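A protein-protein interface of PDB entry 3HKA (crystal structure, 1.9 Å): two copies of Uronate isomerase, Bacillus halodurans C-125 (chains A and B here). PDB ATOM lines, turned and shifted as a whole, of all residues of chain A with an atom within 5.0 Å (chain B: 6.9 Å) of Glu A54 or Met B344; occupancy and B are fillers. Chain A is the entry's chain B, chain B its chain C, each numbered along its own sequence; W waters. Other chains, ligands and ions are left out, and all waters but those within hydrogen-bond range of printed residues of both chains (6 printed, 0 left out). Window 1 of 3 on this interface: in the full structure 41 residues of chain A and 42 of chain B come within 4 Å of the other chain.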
ATOM      1  N   TYR A  50     -16.867 -20.888  10.350  1.00  0.00           N
ATOM      2  CA  TYR A  50     -15.929 -19.769  10.456  1.00  0.00           C
ATOM      3  C   TYR A  50     -16.504 -18.711  11.400  1.00  0.00           C
ATOM      4  O   TYR A  50     -15.787 -18.136  12.219  1.00  0.00           O
ATOM      5  CB  TYR A  50     -15.690 -19.117   9.090  1.00  0.00           C
ATOM      6  CG  TYR A  50     -14.673 -19.802   8.203  1.00  0.00           C
ATOM      7  CD1 TYR A  50     -14.624 -21.186   8.098  1.00  0.00           C
ATOM      8  CD2 TYR A  50     -13.798 -19.054   7.413  1.00  0.00           C
ATOM      9  CE1 TYR A  50     -13.736 -21.814   7.223  1.00  0.00           C
ATOM     10  CE2 TYR A  50     -12.905 -19.671   6.532  1.00  0.00           C
ATOM     11  CZ  TYR A  50     -12.883 -21.050   6.442  1.00  0.00           C
ATOM     12  OH  TYR A  50     -12.020 -21.663   5.562  1.00  0.00           O
ATOM     13  N   LEU A  51     -17.803 -18.450  11.273  1.00  0.00           N
ATOM     14  CA  LEU A  51     -18.456 -17.448  12.104  1.00  0.00           C
ATOM     15  C   LEU A  51     -18.781 -17.955  13.500  1.00  0.00           C
ATOM     16  O   LEU A  51     -18.929 -17.164  14.427  1.00  0.00           O
ATOM     17  CB  LEU A  51     -19.728 -16.928  11.419  1.00  0.00           C
ATOM     18  CG  LEU A  51     -19.518 -15.973  10.235  1.00  0.00           C
ATOM     19  CD1 LEU A  51     -18.765 -16.677   9.127  1.00  0.00           C
ATOM     20  CD2 LEU A  51     -20.858 -15.489   9.720  1.00  0.00           C
ATOM     21  N   VAL A  52     -18.894 -19.269  13.656  1.00  0.00           N
ATOM     22  CA  VAL A  52     -19.172 -19.828  14.971  1.00  0.00           C
ATOM     23  C   VAL A  52     -17.954 -19.540  15.842  1.00  0.00           C
ATOM     24  O   VAL A  52     -18.080 -19.132  16.997  1.00  0.00           O
ATOM     25  CB  VAL A  52     -19.420 -21.350  14.896  1.00  0.00           C
ATOM     26  CG1 VAL A  52     -19.541 -21.941  16.304  1.00  0.00           C
ATOM     27  CG2 VAL A  52     -20.695 -21.622  14.108  1.00  0.00           C
ATOM     28  N   ALA A  53     -16.768 -19.735  15.270  1.00  0.00           N
ATOM     29  CA  ALA A  53     -15.526 -19.484  15.994  1.00  0.00           C
ATOM     30  C   ALA A  53     -15.411 -17.999  16.345  1.00  0.00           C
ATOM     31  O   ALA A  53     -15.033 -17.636  17.458  1.00  0.00           O
ATOM     32  CB  ALA A  53     -14.329 -19.919  15.147  1.00  0.00           C
ATOM     33  N   GLU A  54     -15.761 -17.139  15.395  1.00  0.00           N
ATOM     34  CA  GLU A  54     -15.669 -15.706  15.618  1.00  0.00           C
ATOM     35  C   GLU A  54     -16.675 -15.163  16.630  1.00  0.00           C
ATOM     36  O   GLU A  54     -16.335 -14.310  17.450  1.00  0.00           O
ATOM     37  CB  GLU A  54     -15.790 -14.968  14.281  1.00  0.00           C
ATOM     38  CG  GLU A  54     -14.540 -15.100  13.420  1.00  0.00           C
ATOM     39  CD  GLU A  54     -14.664 -14.400  12.082  1.00  0.00           C
ATOM     40  OE1 GLU A  54     -15.168 -13.255  12.050  1.00  0.00           O
ATOM     41  OE2 GLU A  54     -14.244 -14.991  11.066  1.00  0.00           O
ATOM     42  N   VAL A  55     -17.909 -15.656  16.590  1.00  0.00           N
ATOM     43  CA  VAL A  55     -18.905 -15.169  17.532  1.00  0.00           C
ATOM     44  C   VAL A  55     -18.558 -15.602  18.953  1.00  0.00           C
ATOM     45  O   VAL A  55     -18.819 -14.869  19.907  1.00  0.00           O
ATOM     46  CB  VAL A  55     -20.334 -15.666  17.177  1.00  0.00           C
ATOM     47  CG1 VAL A  55     -20.493 -17.141  17.520  1.00  0.00           C
ATOM     48  CG2 VAL A  55     -21.363 -14.824  17.916  1.00  0.00           C
ATOM     49  N   MET A  56     -17.955 -16.779  19.097  1.00  0.00           N
ATOM     50  CA  MET A  56     -17.601 -17.263  20.429  1.00  0.00           C
ATOM     51  C   MET A  56     -16.536 -16.419  21.125  1.00  0.00           C
ATOM     52  O   MET A  56     -16.320 -16.564  22.323  1.00  0.00           O
ATOM     53  CB  MET A  56     -17.168 -18.730  20.379  1.00  0.00           C
ATOM     54  CG  MET A  56     -18.331 -19.699  20.195  1.00  0.00           C
ATOM     55  SD  MET A  56     -19.662 -19.422  21.415  1.00  0.00           S
ATOM     56  CE  MET A  56     -18.931 -20.090  22.866  1.00  0.00           C
ATOM     57  N   ARG A  57     -15.876 -15.536  20.381  1.00  0.00           N
ATOM     58  CA  ARG A  57     -14.869 -14.662  20.979  1.00  0.00           C
ATOM     59  C   ARG A  57     -15.522 -13.409  21.564  1.00  0.00           C
ATOM     60  O   ARG A  57     -14.884 -12.651  22.300  1.00  0.00           O
ATOM     61  CB  ARG A  57     -13.817 -14.243  19.947  1.00  0.00           C
ATOM     62  CG  ARG A  57     -12.807 -15.333  19.586  1.00  0.00           C
ATOM     63  CD  ARG A  57     -11.638 -14.747  18.797  1.00  0.00           C
ATOM     64  NE  ARG A  57     -10.952 -13.714  19.563  1.00  0.00           N
ATOM     65  CZ  ARG A  57     -10.244 -13.946  20.667  1.00  0.00           C
ATOM     66  NH1 ARG A  57     -10.114 -15.183  21.132  1.00  0.00           N
ATOM     67  NH2 ARG A  57      -9.697 -12.936  21.328  1.00  0.00           N
ATOM     68  N   TRP A  58     -16.796 -13.204  21.241  1.00  0.00           N
ATOM     69  CA  TRP A  58     -17.529 -12.028  21.710  1.00  0.00           C
ATOM     70  C   TRP A  58     -18.723 -12.325  22.620  1.00  0.00           C
ATOM     71  O   TRP A  58     -18.866 -11.723  23.681  1.00  0.00           O
ATOM     72  CB  TRP A  58     -18.054 -11.225  20.514  1.00  0.00           C
ATOM     73  CG  TRP A  58     -17.053 -10.357  19.799  1.00  0.00           C
ATOM     74  CD1 TRP A  58     -16.668 -10.462  18.491  1.00  0.00           C
ATOM     75  CD2 TRP A  58     -16.387  -9.198  20.320  1.00  0.00           C
ATOM     76  NE1 TRP A  58     -15.813  -9.437  18.163  1.00  0.00           N
ATOM     77  CE2 TRP A  58     -15.621  -8.647  19.266  1.00  0.00           C
ATOM     78  CE3 TRP A  58     -16.368  -8.568  21.574  1.00  0.00           C
ATOM     79  CZ2 TRP A  58     -14.841  -7.494  19.427  1.00  0.00           C
ATOM     80  CZ3 TRP A  58     -15.591  -7.420  21.736  1.00  0.00           C
ATOM     81  CH2 TRP A  58     -14.836  -6.895  20.666  1.00  0.00           C
ATOM     82  N   LEU A  82     -21.670 -10.215  15.474  1.00  0.00           N
ATOM     83  CA  LEU A  82     -20.609  -9.894  14.521  1.00  0.00           C
ATOM     84  C   LEU A  82     -20.874  -8.782  13.506  1.00  0.00           C
ATOM     85  O   LEU A  82     -19.935  -8.257  12.905  1.00  0.00           O
ATOM     86  CB  LEU A  82     -20.199 -11.161  13.766  1.00  0.00           C
ATOM     87  CG  LEU A  82     -19.746 -12.350  14.618  1.00  0.00           C
ATOM     88  CD1 LEU A  82     -19.292 -13.484  13.707  1.00  0.00           C
ATOM     89  CD2 LEU A  82     -18.623 -11.924  15.553  1.00  0.00           C
ATOM     90  N   SER A  90     -14.148  -8.695   9.339  1.00  0.00           N
ATOM     91  CA  SER A  90     -13.404  -9.936   9.102  1.00  0.00           C
ATOM     92  C   SER A  90     -13.715 -10.480   7.705  1.00  0.00           C
ATOM     93  O   SER A  90     -14.765 -10.181   7.127  1.00  0.00           O
ATOM     94  CB  SER A  90     -13.757 -10.997  10.156  1.00  0.00           C
ATOM     95  OG  SER A  90     -15.010 -11.603   9.891  1.00  0.00           O
ATOM     96  N   ALA A  92     -14.541 -13.505   6.720  1.00  0.00           N
ATOM     97  CA  ALA A  92     -15.739 -14.336   6.697  1.00  0.00           C
ATOM     98  C   ALA A  92     -17.021 -13.503   6.752  1.00  0.00           C
ATOM     99  O   ALA A  92     -18.012 -13.832   6.086  1.00  0.00           O
ATOM    100  CB  ALA A  92     -15.712 -15.343   7.859  1.00  0.00           C
ATOM    101  N   CYS A  93     -17.005 -12.436   7.546  1.00  0.00           N
ATOM    102  CA  CYS A  93     -18.178 -11.570   7.674  1.00  0.00           C
ATOM    103  C   CYS A  93     -18.360 -10.744   6.408  1.00  0.00           C
ATOM    104  O   CYS A  93     -19.480 -10.560   5.930  1.00  0.00           O
ATOM    105  CB  CYS A  93     -18.036 -10.649   8.889  1.00  0.00           C
ATOM    106  SG  CYS A  93     -18.269 -11.497  10.489  1.00  0.00           S
ATOM    107  N   PHE A 327      -7.253 -21.278   6.703  1.00  0.00           N
ATOM    108  CA  PHE A 327      -6.623 -20.173   7.415  1.00  0.00           C
ATOM    109  C   PHE A 327      -5.702 -19.372   6.501  1.00  0.00           C
ATOM    110  O   PHE A 327      -5.214 -18.307   6.879  1.00  0.00           O
ATOM    111  CB  PHE A 327      -5.877 -20.710   8.643  1.00  0.00           C
ATOM    112  CG  PHE A 327      -6.772 -21.465   9.600  1.00  0.00           C
ATOM    113  CD1 PHE A 327      -7.922 -20.865  10.117  1.00  0.00           C
ATOM    114  CD2 PHE A 327      -6.491 -22.782   9.948  1.00  0.00           C
ATOM    115  CE1 PHE A 327      -8.783 -21.569  10.962  1.00  0.00           C
ATOM    116  CE2 PHE A 327      -7.346 -23.501  10.796  1.00  0.00           C
ATOM    117  CZ  PHE A 327      -8.495 -22.887  11.302  1.00  0.00           C
ATOM    118  N   ASN A 330      -7.275 -15.758   3.254  1.00  0.00           N
ATOM    119  CA  ASN A 330      -7.468 -14.386   3.715  1.00  0.00           C
ATOM    120  C   ASN A 330      -6.638 -13.487   2.787  1.00  0.00           C
ATOM    121  O   ASN A 330      -5.532 -13.853   2.398  1.00  0.00           O
ATOM    122  CB  ASN A 330      -6.980 -14.261   5.161  1.00  0.00           C
ATOM    123  CG  ASN A 330      -7.863 -15.021   6.145  1.00  0.00           C
ATOM    124  OD1 ASN A 330      -8.958 -14.569   6.493  1.00  0.00           O
ATOM    125  ND2 ASN A 330      -7.394 -16.184   6.590  1.00  0.00           N
ATOM    126  N   GLN B 306       3.280 -15.733  14.344  1.00  0.00           N
ATOM    127  CA  GLN B 306       2.126 -14.840  14.268  1.00  0.00           C
ATOM    128  C   GLN B 306       0.827 -15.358  13.669  1.00  0.00           C
ATOM    129  O   GLN B 306      -0.232 -15.194  14.269  1.00  0.00           O
ATOM    130  CB  GLN B 306       2.514 -13.523  13.586  1.00  0.00           C
ATOM    131  CG  GLN B 306       3.661 -12.763  14.277  1.00  0.00           C
ATOM    132  CD  GLN B 306       3.502 -12.650  15.801  1.00  0.00           C
ATOM    133  OE1 GLN B 306       2.396 -12.457  16.317  1.00  0.00           O
ATOM    134  NE2 GLN B 306       4.620 -12.754  16.521  1.00  0.00           N
ATOM    135  N   HIS B 307       0.892 -15.973  12.495  1.00  0.00           N
ATOM    136  CA  HIS B 307      -0.326 -16.468  11.879  1.00  0.00           C
ATOM    137  C   HIS B 307      -0.997 -17.562  12.711  1.00  0.00           C
ATOM    138  O   HIS B 307      -2.209 -17.525  12.926  1.00  0.00           O
ATOM    139  CB  HIS B 307      -0.043 -16.972  10.466  1.00  0.00           C
ATOM    140  CG  HIS B 307      -1.221 -17.634   9.823  1.00  0.00           C
ATOM    141  ND1 HIS B 307      -1.514 -18.967  10.003  1.00  0.00           N
ATOM    142  CD2 HIS B 307      -2.203 -17.135   9.036  1.00  0.00           C
ATOM    143  CE1 HIS B 307      -2.625 -19.263   9.353  1.00  0.00           C
ATOM    144  NE2 HIS B 307      -3.063 -18.168   8.758  1.00  0.00           N
ATOM    145  N   GLU B 308      -0.221 -18.531  13.188  1.00  0.00           N
ATOM    146  CA  GLU B 308      -0.816 -19.602  13.988  1.00  0.00           C
ATOM    147  C   GLU B 308      -1.349 -19.088  15.332  1.00  0.00           C
ATOM    148  O   GLU B 308      -2.281 -19.670  15.892  1.00  0.00           O
ATOM    149  CB  GLU B 308       0.183 -20.752  14.197  1.00  0.00           C
ATOM    150  CG  GLU B 308       1.511 -20.362  14.822  1.00  0.00           C
ATOM    151  CD  GLU B 308       2.534 -21.472  14.703  1.00  0.00           C
ATOM    152  OE1 GLU B 308       2.239 -22.472  14.007  1.00  0.00           O
ATOM    153  OE2 GLU B 308       3.630 -21.343  15.290  1.00  0.00           O
ATOM    154  N   VAL B 310      -2.863 -16.293  15.690  1.00  0.00           N
ATOM    155  CA  VAL B 310      -4.166 -15.756  15.320  1.00  0.00           C
ATOM    156  C   VAL B 310      -5.170 -16.893  15.238  1.00  0.00           C
ATOM    157  O   VAL B 310      -6.271 -16.796  15.772  1.00  0.00           O
ATOM    158  CB  VAL B 310      -4.113 -15.038  13.950  1.00  0.00           C
ATOM    159  CG1 VAL B 310      -5.529 -14.611  13.522  1.00  0.00           C
ATOM    160  CG2 VAL B 310      -3.195 -13.820  14.044  1.00  0.00           C
ATOM    161  N   VAL B 311      -4.784 -17.981  14.578  1.00  0.00           N
ATOM    162  CA  VAL B 311      -5.676 -19.121  14.440  1.00  0.00           C
ATOM    163  C   VAL B 311      -6.055 -19.689  15.803  1.00  0.00           C
ATOM    164  O   VAL B 311      -7.201 -20.096  16.010  1.00  0.00           O
ATOM    165  CB  VAL B 311      -5.043 -20.230  13.577  1.00  0.00           C
ATOM    166  CG1 VAL B 311      -6.003 -21.409  13.455  1.00  0.00           C
ATOM    167  CG2 VAL B 311      -4.718 -19.677  12.193  1.00  0.00           C
ATOM    168  N   ALA B 313      -6.351 -18.035  18.538  1.00  0.00           N
ATOM    169  CA  ALA B 313      -7.317 -17.118  19.139  1.00  0.00           C
ATOM    170  C   ALA B 313      -8.723 -17.432  18.610  1.00  0.00           C
ATOM    171  O   ALA B 313      -9.717 -17.244  19.314  1.00  0.00           O
ATOM    172  CB  ALA B 313      -6.938 -15.674  18.829  1.00  0.00           C
ATOM    173  N   ARG B 314      -8.803 -17.906  17.369  1.00  0.00           N
ATOM    174  CA  ARG B 314     -10.092 -18.263  16.783  1.00  0.00           C
ATOM    175  C   ARG B 314     -10.670 -19.458  17.544  1.00  0.00           C
ATOM    176  O   ARG B 314     -11.890 -19.629  17.623  1.00  0.00           O
ATOM    177  CB  ARG B 314      -9.943 -18.651  15.301  1.00  0.00           C
ATOM    178  CG  ARG B 314      -9.615 -17.510  14.326  1.00  0.00           C
ATOM    179  CD  ARG B 314      -9.590 -18.032  12.879  1.00  0.00           C
ATOM    180  NE  ARG B 314     -10.857 -18.665  12.499  1.00  0.00           N
ATOM    181  CZ  ARG B 314     -11.931 -18.011  12.057  1.00  0.00           C
ATOM    182  NH1 ARG B 314     -11.908 -16.690  11.915  1.00  0.00           N
ATOM    183  NH2 ARG B 314     -13.045 -18.679  11.783  1.00  0.00           N
ATOM    184  N   ARG B 339      -3.133  -7.011   9.726  1.00  0.00           N
ATOM    185  CA  ARG B 339      -4.046  -7.450   8.678  1.00  0.00           C
ATOM    186  C   ARG B 339      -4.480  -8.901   8.865  1.00  0.00           C
ATOM    187  O   ARG B 339      -5.643  -9.223   8.651  1.00  0.00           O
ATOM    188  CB  ARG B 339      -3.412  -7.248   7.300  1.00  0.00           C
ATOM    189  CG  ARG B 339      -3.396  -5.776   6.890  1.00  0.00           C
ATOM    190  CD  ARG B 339      -2.510  -5.492   5.691  1.00  0.00           C
ATOM    191  NE  ARG B 339      -2.511  -4.058   5.392  1.00  0.00           N
ATOM    192  CZ  ARG B 339      -3.507  -3.419   4.782  1.00  0.00           C
ATOM    193  NH1 ARG B 339      -4.587  -4.083   4.386  1.00  0.00           N
ATOM    194  NH2 ARG B 339      -3.433  -2.110   4.589  1.00  0.00           N
ATOM    195  N   MET B 340      -3.561  -9.783   9.255  1.00  0.00           N
ATOM    196  CA  MET B 340      -3.932 -11.183   9.467  1.00  0.00           C
ATOM    197  C   MET B 340      -4.915 -11.277  10.622  1.00  0.00           C
ATOM    198  O   MET B 340      -5.892 -12.021  10.563  1.00  0.00           O
ATOM    199  CB  MET B 340      -2.709 -12.050   9.793  1.00  0.00           C
ATOM    200  CG  MET B 340      -1.787 -12.307   8.617  1.00  0.00           C
ATOM    201  SD  MET B 340      -0.479 -13.478   9.040  1.00  0.00           S
ATOM    202  CE  MET B 340       0.524 -12.486  10.137  1.00  0.00           C
ATOM    203  N   ARG B 341      -4.645 -10.510  11.672  1.00  0.00           N
ATOM    204  CA  ARG B 341      -5.496 -10.504  12.855  1.00  0.00           C
ATOM    205  C   ARG B 341      -6.917 -10.043  12.562  1.00  0.00           C
ATOM    206  O   ARG B 341      -7.879 -10.706  12.941  1.00  0.00           O
ATOM    207  CB  ARG B 341      -4.866  -9.623  13.935  1.00  0.00           C
ATOM    208  CG  ARG B 341      -3.618 -10.246  14.564  1.00  0.00           C
ATOM    209  CD  ARG B 341      -2.849  -9.246  15.397  1.00  0.00           C
ATOM    210  NE  ARG B 341      -1.850  -9.900  16.240  1.00  0.00           N
ATOM    211  CZ  ARG B 341      -1.129  -9.276  17.167  1.00  0.00           C
ATOM    212  NH1 ARG B 341      -1.288  -7.971  17.373  1.00  0.00           N
ATOM    213  NH2 ARG B 341      -0.266  -9.965  17.910  1.00  0.00           N
ATOM    214  N   MET B 342      -7.058  -8.915  11.875  1.00  0.00           N
ATOM    215  CA  MET B 342      -8.391  -8.413  11.574  1.00  0.00           C
ATOM    216  C   MET B 342      -9.144  -9.327  10.604  1.00  0.00           C
ATOM    217  O   MET B 342     -10.347  -9.529  10.744  1.00  0.00           O
ATOM    218  CB  MET B 342      -8.307  -6.986  11.012  1.00  0.00           C
ATOM    219  CG  MET B 342      -9.647  -6.257  10.993  1.00  0.00           C
ATOM    220  SD  MET B 342      -9.479  -4.491  10.657  1.00  0.00           S
ATOM    221  CE  MET B 342      -8.897  -3.903  12.235  1.00  0.00           C
ATOM    222  N   GLU B 343      -8.436  -9.907   9.638  1.00  0.00           N
ATOM    223  CA  GLU B 343      -9.083 -10.778   8.665  1.00  0.00           C
ATOM    224  C   GLU B 343      -9.652 -12.041   9.299  1.00  0.00           C
ATOM    225  O   GLU B 343     -10.684 -12.541   8.857  1.00  0.00           O
ATOM    226  CB  GLU B 343      -8.106 -11.112   7.524  1.00  0.00           C
ATOM    227  CG  GLU B 343      -7.618  -9.832   6.828  1.00  0.00           C
ATOM    228  CD  GLU B 343      -6.667 -10.046   5.655  1.00  0.00           C
ATOM    229  OE1 GLU B 343      -6.078 -11.142   5.513  1.00  0.00           O
ATOM    230  OE2 GLU B 343      -6.495  -9.080   4.879  1.00  0.00           O
ATOM    231  N   MET B 344      -9.001 -12.538  10.353  1.00  0.00           N
ATOM    232  CA  MET B 344      -9.468 -13.745  11.040  1.00  0.00           C
ATOM    233  C   MET B 344     -10.157 -13.518  12.390  1.00  0.00           C
ATOM    234  O   MET B 344     -10.811 -14.426  12.911  1.00  0.00           O
ATOM    235  CB  MET B 344      -8.303 -14.727  11.241  1.00  0.00           C
ATOM    236  CG  MET B 344      -7.935 -15.530  10.002  1.00  0.00           C
ATOM    237  SD  MET B 344      -6.646 -16.762  10.345  1.00  0.00           S
ATOM    238  CE  MET B 344      -5.226 -15.712  10.312  1.00  0.00           C
ATOM    239  N   LEU B 345     -10.016 -12.323  12.958  1.00  0.00           N
ATOM    240  CA  LEU B 345     -10.617 -12.035  14.260  1.00  0.00           C
ATOM    241  C   LEU B 345     -11.505 -10.798  14.270  1.00  0.00           C
ATOM    242  O   LEU B 345     -12.086 -10.457  15.304  1.00  0.00           O
ATOM    243  CB  LEU B 345      -9.523 -11.841  15.318  1.00  0.00           C
ATOM    244  CG  LEU B 345      -8.469 -12.946  15.430  1.00  0.00           C
ATOM    245  CD1 LEU B 345      -7.400 -12.515  16.413  1.00  0.00           C
ATOM    246  CD2 LEU B 345      -9.123 -14.249  15.876  1.00  0.00           C
ATOM    247  N   GLY B 346     -11.615 -10.122  13.133  1.00  0.00           N
ATOM    248  CA  GLY B 346     -12.423  -8.918  13.098  1.00  0.00           C
ATOM    249  C   GLY B 346     -11.795  -7.910  14.044  1.00  0.00           C
ATOM    250  O   GLY B 346     -10.645  -7.516  13.858  1.00  0.00           O
ATOM    251  N   SER B 348     -11.824  -8.481  17.508  1.00  0.00           N
ATOM    252  CA  SER B 348     -11.617  -9.133  18.802  1.00  0.00           C
ATOM    253  C   SER B 348     -10.160  -9.375  19.204  1.00  0.00           C
ATOM    254  O   SER B 348      -9.786 -10.494  19.548  1.00  0.00           O
ATOM    255  CB  SER B 348     -12.397 -10.455  18.868  1.00  0.00           C
ATOM    256  OG  SER B 348     -11.926 -11.400  17.923  1.00  0.00           O
HETATM  257  O   HOH W   1     -13.825 -18.895  19.384  1.00  0.00           O
HETATM  258  O   HOH W   2      -7.219 -11.819  20.393  1.00  0.00           O
HETATM  259  O   HOH W   3     -12.737 -14.344   8.841  1.00  0.00           O
HETATM  260  O   HOH W   4     -15.061  -9.010  15.359  1.00  0.00           O
HETATM  261  O   HOH W   5     -14.807 -11.526  14.061  1.00  0.00           O
HETATM  262  O   HOH W   6     -14.108 -12.806  16.512  1.00  0.00           O
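The guanidinium group (NH1) of Arg A57 lies within hydrogen-bond range of the backbone carbonyl oxygen (O) of Ala B313, at 2.8 Å. OG of Ser B348 lies within hydrogen-bond range of NE of Arg A57 (3.0 Å). O of Phe A327 lies within hydrogen-bond range of NE2 of His B307, 2.9 Å away. OE2 of Glu A54 lies within salt-bridge range of NH1 of Arg B314, at 3.0 Å. The backbone carbonyl oxygen of Tyr A50 is in hydrogen-bond range of the guanidinium group of Arg B314 (2.8 Å).
No position is printed for both chains. Of the 16 pairs that touch across the chains among the printed residues, none has its exchanged pair printed and touching as well.
Water W1 lies within hydrogen-bond range of the backbone carbonyl oxygen of Ala A53 (2.6 Å) and the backbone carbonyl oxygen of Arg B314 (2.7 Å). Water W5 lies within hydrogen-bond range of OE1 of Glu A54 (2.7 Å) and O of Leu B345 (3.2 Å). Water W3 lies within hydrogen-bond range of O of Glu B343, OE2 of Glu A54 and N of Ala A92. Water W6 lies within hydrogen-bond range of the backbone carbonyl oxygen of Glu A54 (2.8 Å), the side-chain hydroxyl of Ser B348 (3.0 Å) and the backbone carbonyl oxygen of Leu B345 (3.3 Å). Water W2 lies within hydrogen-bond range of NH2 of Arg A57 (2.9 Å) and O of Ser B348 (3.0 Å). Water W4 lies within hydrogen-bond range of the indole nitrogen of Trp A58 and the backbone carbonyl oxygen of Leu B345.
Among the printed residues, pairs that only touch across the chains: Ala A53 with Arg B314, Glu A54 with Met B344, Arg A57 with Leu B345, Trp A58 with Ser B348, Ser A90 with Met B342, Ser A90 with Glu B343, Ser A90 with Gly B346, Phe A327 with Val B311, Phe A327 with Arg B314, Asn A330 with Glu B343 and Asn A330 with Met B344.
Of chain A, only Glu A54 and Asn A330 come within 4 Å of Met B344. Printed residues of chain B within 4 Å of Trp A58: Ser B348. Of the printed residues of chain A, Ala B313 touches Arg A57. Of the printed residues of chain A, Leu B345 touches Arg A57. Of the printed residues of chain A, Gly B346 touches Ser A90. The nearest printed residue of chain B that does not touch Glu A54 is Glu B343 (4.9 Å). The nearest residue of chain A that does not touch Met B344 is Phe A327 (4.1 Å).
Of the 16 printed residues of chain B, 10 touch a printed residue of chain A. Printed residues of chain B that touch a printed residue of chain A: His B307, Val B311, Ala B313, Arg B314, Met B342, Glu B343, Met B344, Leu B345, Gly B346 and Ser B348. Hydrophobic or aromatic side chains of chain B that line the printed part of chain A: His B307, Val B311, Ala B313, Met B344 and Leu B345. Hydrophobic or aromatic side chains of chain A within 4 Å of the printed part of chain B: Tyr A50, Ala A53, Trp A58 and Phe A327.
OG of Ser B348 lies within hydrogen-bond range of O of Leu B345 (2.8 Å). O of Met B344 lies within hydrogen-bond range of NH1 of Arg B314 (2.7 Å). ND2 of Asn A330 sits at hydrogen-bond distance from O of Phe A327, 3.1 Å away. OG of Ser A90 sits at hydrogen-bond distance from N of Cys A93 (3.2 Å). The side-chain hydroxyl of Ser A90 sits at hydrogen-bond distance from the side-chain carboxylate of Glu A54 (2.7 Å).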
